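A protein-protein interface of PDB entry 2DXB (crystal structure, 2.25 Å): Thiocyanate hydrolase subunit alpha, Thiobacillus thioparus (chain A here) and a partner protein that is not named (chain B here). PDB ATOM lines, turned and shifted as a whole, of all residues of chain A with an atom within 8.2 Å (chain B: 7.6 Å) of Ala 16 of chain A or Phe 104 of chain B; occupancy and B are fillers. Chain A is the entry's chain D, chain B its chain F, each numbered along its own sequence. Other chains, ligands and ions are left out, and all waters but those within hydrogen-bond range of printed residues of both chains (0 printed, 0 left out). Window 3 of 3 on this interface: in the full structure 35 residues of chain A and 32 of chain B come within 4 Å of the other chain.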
ATOM      1  N   ASP A  11      -0.916  36.663 -15.362  1.00  0.00           N
ATOM      2  CA  ASP A  11      -1.615  35.841 -14.385  1.00  0.00           C
ATOM      3  C   ASP A  11      -2.261  34.661 -15.102  1.00  0.00           C
ATOM      4  O   ASP A  11      -3.299  34.810 -15.748  1.00  0.00           O
ATOM      5  CB  ASP A  11      -2.690  36.675 -13.686  1.00  0.00           C
ATOM      6  CG  ASP A  11      -3.401  35.910 -12.594  1.00  0.00           C
ATOM      7  OD1 ASP A  11      -3.151  34.692 -12.458  1.00  0.00           O
ATOM      8  OD2 ASP A  11      -4.214  36.529 -11.875  1.00  0.00           O
ATOM      9  N   ARG A  12      -1.652  33.490 -14.978  1.00  0.00           N
ATOM     10  CA  ARG A  12      -2.162  32.300 -15.639  1.00  0.00           C
ATOM     11  C   ARG A  12      -3.133  31.447 -14.827  1.00  0.00           C
ATOM     12  O   ARG A  12      -3.543  30.386 -15.286  1.00  0.00           O
ATOM     13  CB  ARG A  12      -0.992  31.434 -16.100  1.00  0.00           C
ATOM     14  CG  ARG A  12      -0.236  31.992 -17.289  1.00  0.00           C
ATOM     15  CD  ARG A  12       0.915  31.079 -17.647  1.00  0.00           C
ATOM     16  NE  ARG A  12       2.072  31.321 -16.796  1.00  0.00           N
ATOM     17  CZ  ARG A  12       2.983  30.404 -16.491  1.00  0.00           C
ATOM     18  NH1 ARG A  12       2.875  29.166 -16.960  1.00  0.00           N
ATOM     19  NH2 ARG A  12       4.017  30.734 -15.729  1.00  0.00           N
ATOM     20  N   THR A  13      -3.509  31.893 -13.633  1.00  0.00           N
ATOM     21  CA  THR A  13      -4.432  31.111 -12.813  1.00  0.00           C
ATOM     22  C   THR A  13      -5.805  31.761 -12.677  1.00  0.00           C
ATOM     23  O   THR A  13      -6.757  31.116 -12.247  1.00  0.00           O
ATOM     24  CB  THR A  13      -3.885  30.888 -11.381  1.00  0.00           C
ATOM     25  OG1 THR A  13      -3.837  32.140 -10.686  1.00  0.00           O
ATOM     26  CG2 THR A  13      -2.492  30.285 -11.425  1.00  0.00           C
ATOM     27  N   HIS A  14      -5.912  33.031 -13.049  1.00  0.00           N
ATOM     28  CA  HIS A  14      -7.178  33.747 -12.926  1.00  0.00           C
ATOM     29  C   HIS A  14      -8.408  33.070 -13.525  1.00  0.00           C
ATOM     30  O   HIS A  14      -9.414  32.895 -12.840  1.00  0.00           O
ATOM     31  CB  HIS A  14      -7.070  35.148 -13.520  1.00  0.00           C
ATOM     32  CG  HIS A  14      -8.381  35.868 -13.573  1.00  0.00           C
ATOM     33  ND1 HIS A  14      -9.075  36.231 -12.438  1.00  0.00           N
ATOM     34  CD2 HIS A  14      -9.150  36.244 -14.622  1.00  0.00           C
ATOM     35  CE1 HIS A  14     -10.216  36.799 -12.787  1.00  0.00           C
ATOM     36  NE2 HIS A  14     -10.286  36.819 -14.106  1.00  0.00           N
ATOM     37  N   HIS A  15      -8.344  32.708 -14.802  1.00  0.00           N
ATOM     38  CA  HIS A  15      -9.494  32.082 -15.448  1.00  0.00           C
ATOM     39  C   HIS A  15      -9.918  30.778 -14.777  1.00  0.00           C
ATOM     40  O   HIS A  15     -11.103  30.564 -14.517  1.00  0.00           O
ATOM     41  CB  HIS A  15      -9.213  31.817 -16.927  1.00  0.00           C
ATOM     42  CG  HIS A  15     -10.413  31.339 -17.681  1.00  0.00           C
ATOM     43  ND1 HIS A  15     -11.488  32.155 -17.960  1.00  0.00           N
ATOM     44  CD2 HIS A  15     -10.740  30.115 -18.159  1.00  0.00           C
ATOM     45  CE1 HIS A  15     -12.424  31.456 -18.574  1.00  0.00           C
ATOM     46  NE2 HIS A  15     -11.996  30.213 -18.706  1.00  0.00           N
ATOM     47  N   ALA A  16      -8.949  29.911 -14.500  1.00  0.00           N
ATOM     48  CA  ALA A  16      -9.232  28.626 -13.873  1.00  0.00           C
ATOM     49  C   ALA A  16      -9.806  28.757 -12.463  1.00  0.00           C
ATOM     50  O   ALA A  16     -10.704  28.007 -12.083  1.00  0.00           O
ATOM     51  CB  ALA A  16      -7.969  27.773 -13.842  1.00  0.00           C
ATOM     52  N   LYS A  17      -9.290  29.698 -11.683  1.00  0.00           N
ATOM     53  CA  LYS A  17      -9.779  29.886 -10.322  1.00  0.00           C
ATOM     54  C   LYS A  17     -11.214  30.392 -10.354  1.00  0.00           C
ATOM     55  O   LYS A  17     -12.018  30.080  -9.482  1.00  0.00           O
ATOM     56  CB  LYS A  17      -8.907  30.896  -9.568  1.00  0.00           C
ATOM     57  CG  LYS A  17      -7.498  30.411  -9.270  1.00  0.00           C
ATOM     58  CD  LYS A  17      -6.685  31.480  -8.546  1.00  0.00           C
ATOM     59  CE  LYS A  17      -5.288  30.976  -8.221  1.00  0.00           C
ATOM     60  NZ  LYS A  17      -4.446  32.023  -7.581  1.00  0.00           N
ATOM     61  N   MET A  18     -11.526  31.166 -11.382  1.00  0.00           N
ATOM     62  CA  MET A  18     -12.847  31.748 -11.539  1.00  0.00           C
ATOM     63  C   MET A  18     -13.920  30.828 -12.125  1.00  0.00           C
ATOM     64  O   MET A  18     -15.070  30.843 -11.681  1.00  0.00           O
ATOM     65  CB  MET A  18     -12.730  33.000 -12.409  1.00  0.00           C
ATOM     66  CG  MET A  18     -14.050  33.535 -12.923  1.00  0.00           C
ATOM     67  SD  MET A  18     -13.818  35.031 -13.884  1.00  0.00           S
ATOM     68  CE  MET A  18     -14.150  36.280 -12.636  1.00  0.00           C
ATOM     69  N   ALA A  19     -13.549  30.025 -13.113  1.00  0.00           N
ATOM     70  CA  ALA A  19     -14.518  29.165 -13.776  1.00  0.00           C
ATOM     71  C   ALA A  19     -14.581  27.706 -13.348  1.00  0.00           C
ATOM     72  O   ALA A  19     -15.561  27.022 -13.654  1.00  0.00           O
ATOM     73  CB  ALA A  19     -14.305  29.242 -15.282  1.00  0.00           C
ATOM     74  N   THR A  20     -13.558  27.224 -12.650  1.00  0.00           N
ATOM     75  CA  THR A  20     -13.542  25.824 -12.240  1.00  0.00           C
ATOM     76  C   THR A  20     -14.790  25.408 -11.479  1.00  0.00           C
ATOM     77  O   THR A  20     -15.192  26.062 -10.521  1.00  0.00           O
ATOM     78  CB  THR A  20     -12.302  25.494 -11.383  1.00  0.00           C
ATOM     79  OG1 THR A  20     -11.126  25.591 -12.192  1.00  0.00           O
ATOM     80  CG2 THR A  20     -12.400  24.081 -10.827  1.00  0.00           C
ATOM     81  N   GLY A  21     -15.397  24.310 -11.924  1.00  0.00           N
ATOM     82  CA  GLY A  21     -16.599  23.800 -11.289  1.00  0.00           C
ATOM     83  C   GLY A  21     -17.835  24.620 -11.609  1.00  0.00           C
ATOM     84  O   GLY A  21     -18.949  24.271 -11.202  1.00  0.00           O
ATOM     85  N   ILE A  22     -17.648  25.704 -12.355  1.00  0.00           N
ATOM     86  CA  ILE A  22     -18.752  26.590 -12.705  1.00  0.00           C
ATOM     87  C   ILE A  22     -19.012  26.643 -14.210  1.00  0.00           C
ATOM     88  O   ILE A  22     -20.141  26.465 -14.659  1.00  0.00           O
ATOM     89  CB  ILE A  22     -18.473  28.020 -12.188  1.00  0.00           C
ATOM     90  CG1 ILE A  22     -18.318  27.990 -10.664  1.00  0.00           C
ATOM     91  CG2 ILE A  22     -19.588  28.961 -12.601  1.00  0.00           C
ATOM     92  CD1 ILE A  22     -17.943  29.332 -10.054  1.00  0.00           C
ATOM     93  N   GLY A  23     -17.960  26.892 -14.983  1.00  0.00           N
ATOM     94  CA  GLY A  23     -18.114  26.966 -16.421  1.00  0.00           C
ATOM     95  C   GLY A  23     -18.057  28.388 -16.954  1.00  0.00           C
ATOM     96  O   GLY A  23     -18.120  29.360 -16.198  1.00  0.00           O
ATOM     97  N   ASP A  24     -17.937  28.492 -18.271  1.00  0.00           N
ATOM     98  CA  ASP A  24     -17.870  29.767 -18.980  1.00  0.00           C
ATOM     99  C   ASP A  24     -18.965  29.645 -20.043  1.00  0.00           C
ATOM    100  O   ASP A  24     -19.000  28.661 -20.785  1.00  0.00           O
ATOM    101  CB  ASP A  24     -16.490  29.882 -19.645  1.00  0.00           C
ATOM    102  CG  ASP A  24     -16.268  31.208 -20.353  1.00  0.00           C
ATOM    103  OD1 ASP A  24     -17.237  31.964 -20.585  1.00  0.00           O
ATOM    104  OD2 ASP A  24     -15.095  31.484 -20.690  1.00  0.00           O
ATOM    105  N   PRO A  25     -19.857  30.641 -20.158  1.00  0.00           N
ATOM    106  CA  PRO A  25     -19.984  31.920 -19.453  1.00  0.00           C
ATOM    107  C   PRO A  25     -20.680  31.924 -18.085  1.00  0.00           C
ATOM    108  O   PRO A  25     -20.905  32.996 -17.524  1.00  0.00           O
ATOM    109  CB  PRO A  25     -20.742  32.771 -20.457  1.00  0.00           C
ATOM    110  CG  PRO A  25     -21.740  31.783 -20.982  1.00  0.00           C
ATOM    111  CD  PRO A  25     -20.887  30.539 -21.213  1.00  0.00           C
ATOM    112  N   GLN A  26     -21.023  30.757 -17.549  1.00  0.00           N
ATOM    113  CA  GLN A  26     -21.697  30.715 -16.252  1.00  0.00           C
ATOM    114  C   GLN A  26     -20.963  31.495 -15.164  1.00  0.00           C
ATOM    115  O   GLN A  26     -21.591  32.036 -14.253  1.00  0.00           O
ATOM    116  CB  GLN A  26     -21.900  29.270 -15.778  1.00  0.00           C
ATOM    117  CG  GLN A  26     -22.904  28.472 -16.599  1.00  0.00           C
ATOM    118  CD  GLN A  26     -22.266  27.739 -17.764  1.00  0.00           C
ATOM    119  OE1 GLN A  26     -21.319  28.228 -18.388  1.00  0.00           O
ATOM    120  NE2 GLN A  26     -22.793  26.559 -18.073  1.00  0.00           N
ATOM    121  N   CYS A  27     -19.638  31.564 -15.260  1.00  0.00           N
ATOM    122  CA  CYS A  27     -18.851  32.272 -14.254  1.00  0.00           C
ATOM    123  C   CYS A  27     -19.061  33.783 -14.254  1.00  0.00           C
ATOM    124  O   CYS A  27     -18.651  34.463 -13.314  1.00  0.00           O
ATOM    125  CB  CYS A  27     -17.357  31.956 -14.421  1.00  0.00           C
ATOM    126  SG  CYS A  27     -16.642  32.403 -16.026  1.00  0.00           S
ATOM    127  N   TRP B  52      -5.327  15.579 -22.962  1.00  0.00           N
ATOM    128  CA  TRP B  52      -6.241  16.244 -23.879  1.00  0.00           C
ATOM    129  C   TRP B  52      -6.498  15.400 -25.117  1.00  0.00           C
ATOM    130  O   TRP B  52      -7.634  15.303 -25.582  1.00  0.00           O
ATOM    131  CB  TRP B  52      -5.727  17.621 -24.298  1.00  0.00           C
ATOM    132  CG  TRP B  52      -6.860  18.451 -24.793  1.00  0.00           C
ATOM    133  CD1 TRP B  52      -7.397  18.445 -26.052  1.00  0.00           C
ATOM    134  CD2 TRP B  52      -7.722  19.270 -23.996  1.00  0.00           C
ATOM    135  NE1 TRP B  52      -8.544  19.198 -26.081  1.00  0.00           N
ATOM    136  CE2 TRP B  52      -8.768  19.717 -24.833  1.00  0.00           C
ATOM    137  CE3 TRP B  52      -7.716  19.664 -22.650  1.00  0.00           C
ATOM    138  CZ2 TRP B  52      -9.803  20.541 -24.369  1.00  0.00           C
ATOM    139  CZ3 TRP B  52      -8.748  20.486 -22.184  1.00  0.00           C
ATOM    140  CH2 TRP B  52      -9.775  20.913 -23.046  1.00  0.00           C
ATOM    141  N   TRP B  96     -21.028  19.451 -19.971  1.00  0.00           N
ATOM    142  CA  TRP B  96     -20.213  20.487 -20.588  1.00  0.00           C
ATOM    143  C   TRP B  96     -19.203  21.164 -19.678  1.00  0.00           C
ATOM    144  O   TRP B  96     -18.228  21.738 -20.155  1.00  0.00           O
ATOM    145  CB  TRP B  96     -21.117  21.531 -21.257  1.00  0.00           C
ATOM    146  CG  TRP B  96     -21.717  21.004 -22.526  1.00  0.00           C
ATOM    147  CD1 TRP B  96     -22.552  19.930 -22.647  1.00  0.00           C
ATOM    148  CD2 TRP B  96     -21.440  21.449 -23.862  1.00  0.00           C
ATOM    149  NE1 TRP B  96     -22.803  19.669 -23.971  1.00  0.00           N
ATOM    150  CE2 TRP B  96     -22.132  20.585 -24.741  1.00  0.00           C
ATOM    151  CE3 TRP B  96     -20.670  22.487 -24.403  1.00  0.00           C
ATOM    152  CZ2 TRP B  96     -22.080  20.727 -26.137  1.00  0.00           C
ATOM    153  CZ3 TRP B  96     -20.616  22.632 -25.794  1.00  0.00           C
ATOM    154  CH2 TRP B  96     -21.317  21.751 -26.642  1.00  0.00           C
ATOM    155  N   VAL B  97     -19.415  21.085 -18.372  1.00  0.00           N
ATOM    156  CA  VAL B  97     -18.498  21.720 -17.437  1.00  0.00           C
ATOM    157  C   VAL B  97     -17.435  20.765 -16.894  1.00  0.00           C
ATOM    158  O   VAL B  97     -16.243  21.091 -16.879  1.00  0.00           O
ATOM    159  CB  VAL B  97     -19.273  22.340 -16.249  1.00  0.00           C
ATOM    160  CG1 VAL B  97     -18.300  22.974 -15.261  1.00  0.00           C
ATOM    161  CG2 VAL B  97     -20.265  23.381 -16.761  1.00  0.00           C
ATOM    162  N   THR B  98     -17.869  19.575 -16.485  1.00  0.00           N
ATOM    163  CA  THR B  98     -16.974  18.589 -15.889  1.00  0.00           C
ATOM    164  C   THR B  98     -16.428  17.452 -16.755  1.00  0.00           C
ATOM    165  O   THR B  98     -15.472  16.793 -16.352  1.00  0.00           O
ATOM    166  CB  THR B  98     -17.630  17.955 -14.660  1.00  0.00           C
ATOM    167  OG1 THR B  98     -18.803  17.242 -15.065  1.00  0.00           O
ATOM    168  CG2 THR B  98     -18.026  19.033 -13.655  1.00  0.00           C
ATOM    169  N   SER B  99     -17.020  17.193 -17.916  1.00  0.00           N
ATOM    170  CA  SER B  99     -16.499  16.122 -18.766  1.00  0.00           C
ATOM    171  C   SER B  99     -15.101  16.467 -19.302  1.00  0.00           C
ATOM    172  O   SER B  99     -14.215  15.619 -19.313  1.00  0.00           O
ATOM    173  CB  SER B  99     -17.459  15.825 -19.925  1.00  0.00           C
ATOM    174  OG  SER B  99     -18.621  15.148 -19.467  1.00  0.00           O
ATOM    175  N   PRO B 100     -14.886  17.715 -19.761  1.00  0.00           N
ATOM    176  CA  PRO B 100     -13.552  18.074 -20.270  1.00  0.00           C
ATOM    177  C   PRO B 100     -12.547  18.071 -19.108  1.00  0.00           C
ATOM    178  O   PRO B 100     -12.928  18.252 -17.954  1.00  0.00           O
ATOM    179  CB  PRO B 100     -13.758  19.479 -20.839  1.00  0.00           C
ATOM    180  CG  PRO B 100     -15.227  19.508 -21.185  1.00  0.00           C
ATOM    181  CD  PRO B 100     -15.847  18.806 -20.003  1.00  0.00           C
ATOM    182  N   PRO B 101     -11.254  17.879 -19.400  1.00  0.00           N
ATOM    183  CA  PRO B 101     -10.205  17.851 -18.371  1.00  0.00           C
ATOM    184  C   PRO B 101     -10.048  19.119 -17.525  1.00  0.00           C
ATOM    185  O   PRO B 101      -9.540  19.065 -16.407  1.00  0.00           O
ATOM    186  CB  PRO B 101      -8.941  17.550 -19.175  1.00  0.00           C
ATOM    187  CG  PRO B 101      -9.463  16.748 -20.331  1.00  0.00           C
ATOM    188  CD  PRO B 101     -10.699  17.522 -20.717  1.00  0.00           C
ATOM    189  N   THR B 102     -10.481  20.254 -18.062  1.00  0.00           N
ATOM    190  CA  THR B 102     -10.368  21.535 -17.370  1.00  0.00           C
ATOM    191  C   THR B 102     -11.233  21.667 -16.125  1.00  0.00           C
ATOM    192  O   THR B 102     -10.831  22.289 -15.149  1.00  0.00           O
ATOM    193  CB  THR B 102     -10.790  22.692 -18.280  1.00  0.00           C
ATOM    194  OG1 THR B 102     -12.185  22.545 -18.588  1.00  0.00           O
ATOM    195  CG2 THR B 102      -9.968  22.707 -19.571  1.00  0.00           C
ATOM    196  N   GLN B 103     -12.434  21.104 -16.187  1.00  0.00           N
ATOM    197  CA  GLN B 103     -13.414  21.188 -15.110  1.00  0.00           C
ATOM    198  C   GLN B 103     -14.128  22.538 -15.171  1.00  0.00           C
ATOM    199  O   GLN B 103     -14.801  22.943 -14.223  1.00  0.00           O
ATOM    200  CB  GLN B 103     -12.772  20.980 -13.738  1.00  0.00           C
ATOM    201  CG  GLN B 103     -12.263  19.562 -13.529  1.00  0.00           C
ATOM    202  CD  GLN B 103     -13.303  18.514 -13.894  1.00  0.00           C
ATOM    203  OE1 GLN B 103     -14.354  18.421 -13.264  1.00  0.00           O
ATOM    204  NE2 GLN B 103     -13.014  17.721 -14.923  1.00  0.00           N
ATOM    205  N   PHE B 104     -13.954  23.243 -16.288  1.00  0.00           N
ATOM    206  CA  PHE B 104     -14.642  24.514 -16.507  1.00  0.00           C
ATOM    207  C   PHE B 104     -15.046  24.600 -17.981  1.00  0.00           C
ATOM    208  O   PHE B 104     -15.243  25.681 -18.537  1.00  0.00           O
ATOM    209  CB  PHE B 104     -13.789  25.726 -16.059  1.00  0.00           C
ATOM    210  CG  PHE B 104     -12.445  25.863 -16.751  1.00  0.00           C
ATOM    211  CD1 PHE B 104     -12.356  26.222 -18.096  1.00  0.00           C
ATOM    212  CD2 PHE B 104     -11.263  25.704 -16.026  1.00  0.00           C
ATOM    213  CE1 PHE B 104     -11.112  26.424 -18.707  1.00  0.00           C
ATOM    214  CE2 PHE B 104     -10.014  25.903 -16.625  1.00  0.00           C
ATOM    215  CZ  PHE B 104      -9.938  26.264 -17.965  1.00  0.00           C
ATOM    216  N   GLY B 105     -15.205  23.419 -18.581  1.00  0.00           N
ATOM    217  CA  GLY B 105     -15.567  23.300 -19.984  1.00  0.00           C
ATOM    218  C   GLY B 105     -14.330  23.435 -20.852  1.00  0.00           C
ATOM    219  O   GLY B 105     -13.309  23.951 -20.390  1.00  0.00           O
ATOM    220  N   THR B 106     -14.387  22.968 -22.097  1.00  0.00           N
ATOM    221  CA  THR B 106     -13.224  23.118 -22.965  1.00  0.00           C
ATOM    222  C   THR B 106     -13.072  24.617 -23.189  1.00  0.00           C
ATOM    223  O   THR B 106     -14.053  25.357 -23.180  1.00  0.00           O
ATOM    224  CB  THR B 106     -13.403  22.434 -24.338  1.00  0.00           C
ATOM    225  OG1 THR B 106     -14.432  23.105 -25.072  1.00  0.00           O
ATOM    226  CG2 THR B 106     -13.763  20.960 -24.164  1.00  0.00           C
ATOM    227  N   PRO B 107     -11.837  25.089 -23.377  1.00  0.00           N
ATOM    228  CA  PRO B 107     -11.614  26.519 -23.595  1.00  0.00           C
ATOM    229  C   PRO B 107     -12.285  27.075 -24.851  1.00  0.00           C
ATOM    230  O   PRO B 107     -12.745  28.215 -24.857  1.00  0.00           O
ATOM    231  CB  PRO B 107     -10.092  26.620 -23.685  1.00  0.00           C
ATOM    232  CG  PRO B 107      -9.624  25.491 -22.815  1.00  0.00           C
ATOM    233  CD  PRO B 107     -10.560  24.373 -23.203  1.00  0.00           C
ATOM    234  N   SER B 108     -12.351  26.265 -25.904  1.00  0.00           N
ATOM    235  CA  SER B 108     -12.915  26.714 -27.175  1.00  0.00           C
ATOM    236  C   SER B 108     -14.391  26.457 -27.452  1.00  0.00           C
ATOM    237  O   SER B 108     -14.966  27.090 -28.341  1.00  0.00           O
ATOM    238  CB  SER B 108     -12.092  26.133 -28.333  1.00  0.00           C
ATOM    239  OG  SER B 108     -10.751  26.595 -28.296  1.00  0.00           O
ATOM    240  N   TYR B 110     -16.796  26.247 -24.780  1.00  0.00           N
ATOM    241  CA  TYR B 110     -17.575  26.859 -23.705  1.00  0.00           C
ATOM    242  C   TYR B 110     -18.640  25.937 -23.120  1.00  0.00           C
ATOM    243  O   TYR B 110     -18.627  24.725 -23.355  1.00  0.00           O
ATOM    244  CB  TYR B 110     -18.214  28.152 -24.206  1.00  0.00           C
ATOM    245  CG  TYR B 110     -17.185  29.123 -24.718  1.00  0.00           C
ATOM    246  CD1 TYR B 110     -16.277  29.733 -23.846  1.00  0.00           C
ATOM    247  CD2 TYR B 110     -17.060  29.375 -26.083  1.00  0.00           C
ATOM    248  CE1 TYR B 110     -15.267  30.565 -24.326  1.00  0.00           C
ATOM    249  CE2 TYR B 110     -16.057  30.200 -26.572  1.00  0.00           C
ATOM    250  CZ  TYR B 110     -15.164  30.790 -25.693  1.00  0.00           C
ATOM    251  OH  TYR B 110     -14.168  31.595 -26.190  1.00  0.00           O
ATOM    252  N   CYS B 111     -19.567  26.520 -22.365  1.00  0.00           N
ATOM    253  CA  CYS B 111     -20.609  25.744 -21.711  1.00  0.00           C
ATOM    254  C   CYS B 111     -22.044  26.242 -21.935  1.00  0.00           C
ATOM    255  O   CYS B 111     -22.815  26.364 -20.981  1.00  0.00           O
ATOM    256  CB  CYS B 111     -20.319  25.688 -20.206  1.00  0.00           C
ATOM    257  SG  CYS B 111     -18.601  25.233 -19.809  1.00  0.00           S
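O of Gln 103 of chain B lies within hydrogen-bond range of N of Gly 21 of chain A (2.7 Å). N of Cys 111 of chain B sits at hydrogen-bond distance from O of Asp 24 of chain A, at 2.7 Å. The side-chain amide nitrogen (NE2) of Gln 26 of chain A is in hydrogen-bond range of the backbone carbonyl oxygen (O) of Cys 111 of chain B, at 2.9 Å.
SG of Cys 27 of chain A lies close to O of Gly 23 of chain A (3.4 Å). O of Asp 24 of chain A sits close to OE1 of Gln 26 of chain A, 3.4 Å away. O of Val 97 of chain B lies within hydrogen-bond range of N of Gly 105 of chain B, at 3.1 Å. The backbone carbonyl oxygen of Thr 98 of chain B sits at hydrogen-bond distance from the side-chain amide nitrogen of Gln 103 of chain B. The side-chain hydroxyl (OG1) of Thr 102 of chain B is in hydrogen-bond range of the backbone NH (N) of Phe 104 of chain B, 3.0 Å away. SG of Cys 111 of chain B lies within hydrogen-bond range of O of Phe 104 of chain B, at 3.6 Å.
CE1 of Phe 104 of chain B touches CD2 of His 15 of chain A, 3.7 Å away. Ala 16 of chain A touches Phe 104 of chain B (CB to CE2, 3.9 Å). O of Ala 19 of chain A touches CB of Phe 104 of chain B, at 3.3 Å. Gln 103 of chain B touches Thr 20 of chain A (O to C, 3.7 Å). N of Thr 20 of chain A touches CB of Phe 104 of chain B, at 3.7 Å. Val 97 of chain B touches Ile 22 of chain A. Gly 23 of chain A touches Val 97 of chain B (N to CG1, 3.9 Å). Gly 23 of chain A touches Phe 104 of chain B. CA of Gly 23 of chain A touches SG of Cys 111 of chain B, at 3.8 Å. O of Phe 104 of chain B touches N of Asp 24 of chain A, at 3.9 Å.
Of the printed residues of chain B, His 15 of chain A touches Phe 104. Of chain B, only Phe 104 (3.9 Å) comes within 4 Å of Ala 16 of chain A. Printed residues of chain B within 4 Å of Ile 22 of chain A: Val 97. Of the printed residues of chain B, Gly 23 of chain A touches Val 97, Phe 104 and Cys 111. Of the printed residues of chain A, Gln 103 of chain B touches Thr 20 and Gly 21. Of the printed residues of chain A, Phe 104 of chain B touches His 15 (3.7 Å), Ala 16 (3.9 Å), Ala 19 (3.3 Å), Thr 20 (3.7 Å), Gly 23 (3.8 Å) and Asp 24 (3.9 Å). No residue of chain A comes within 4 Å of Gly 105 of chain B. Printed residues of chain A within 4 Å of Cys 111 of chain B: Gly 23 (3.8 Å), Asp 24 (2.7 Å) and Gln 26 (2.9 Å).
Of the 16 printed residues of chain B, 5 touch a printed residue of chain A. Printed residues of chain B that touch a printed residue of chain A: Val 97, Gln 103, Phe 104, Tyr 110 and Cys 111. Hydrophobic or aromatic side chains of chain B within 4 Å of the printed part of chain A: Val 97, Phe 104 and Tyr 110. Of the 17 printed residues of chain A, 9 touch a printed residue of chain B. Hydrophobic or aromatic side chains of chain A within 4 Å of the printed part of chain B: His 15, Ala 16 and Ala 19. Among the printed residues, 14 pairs touch across the chains.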
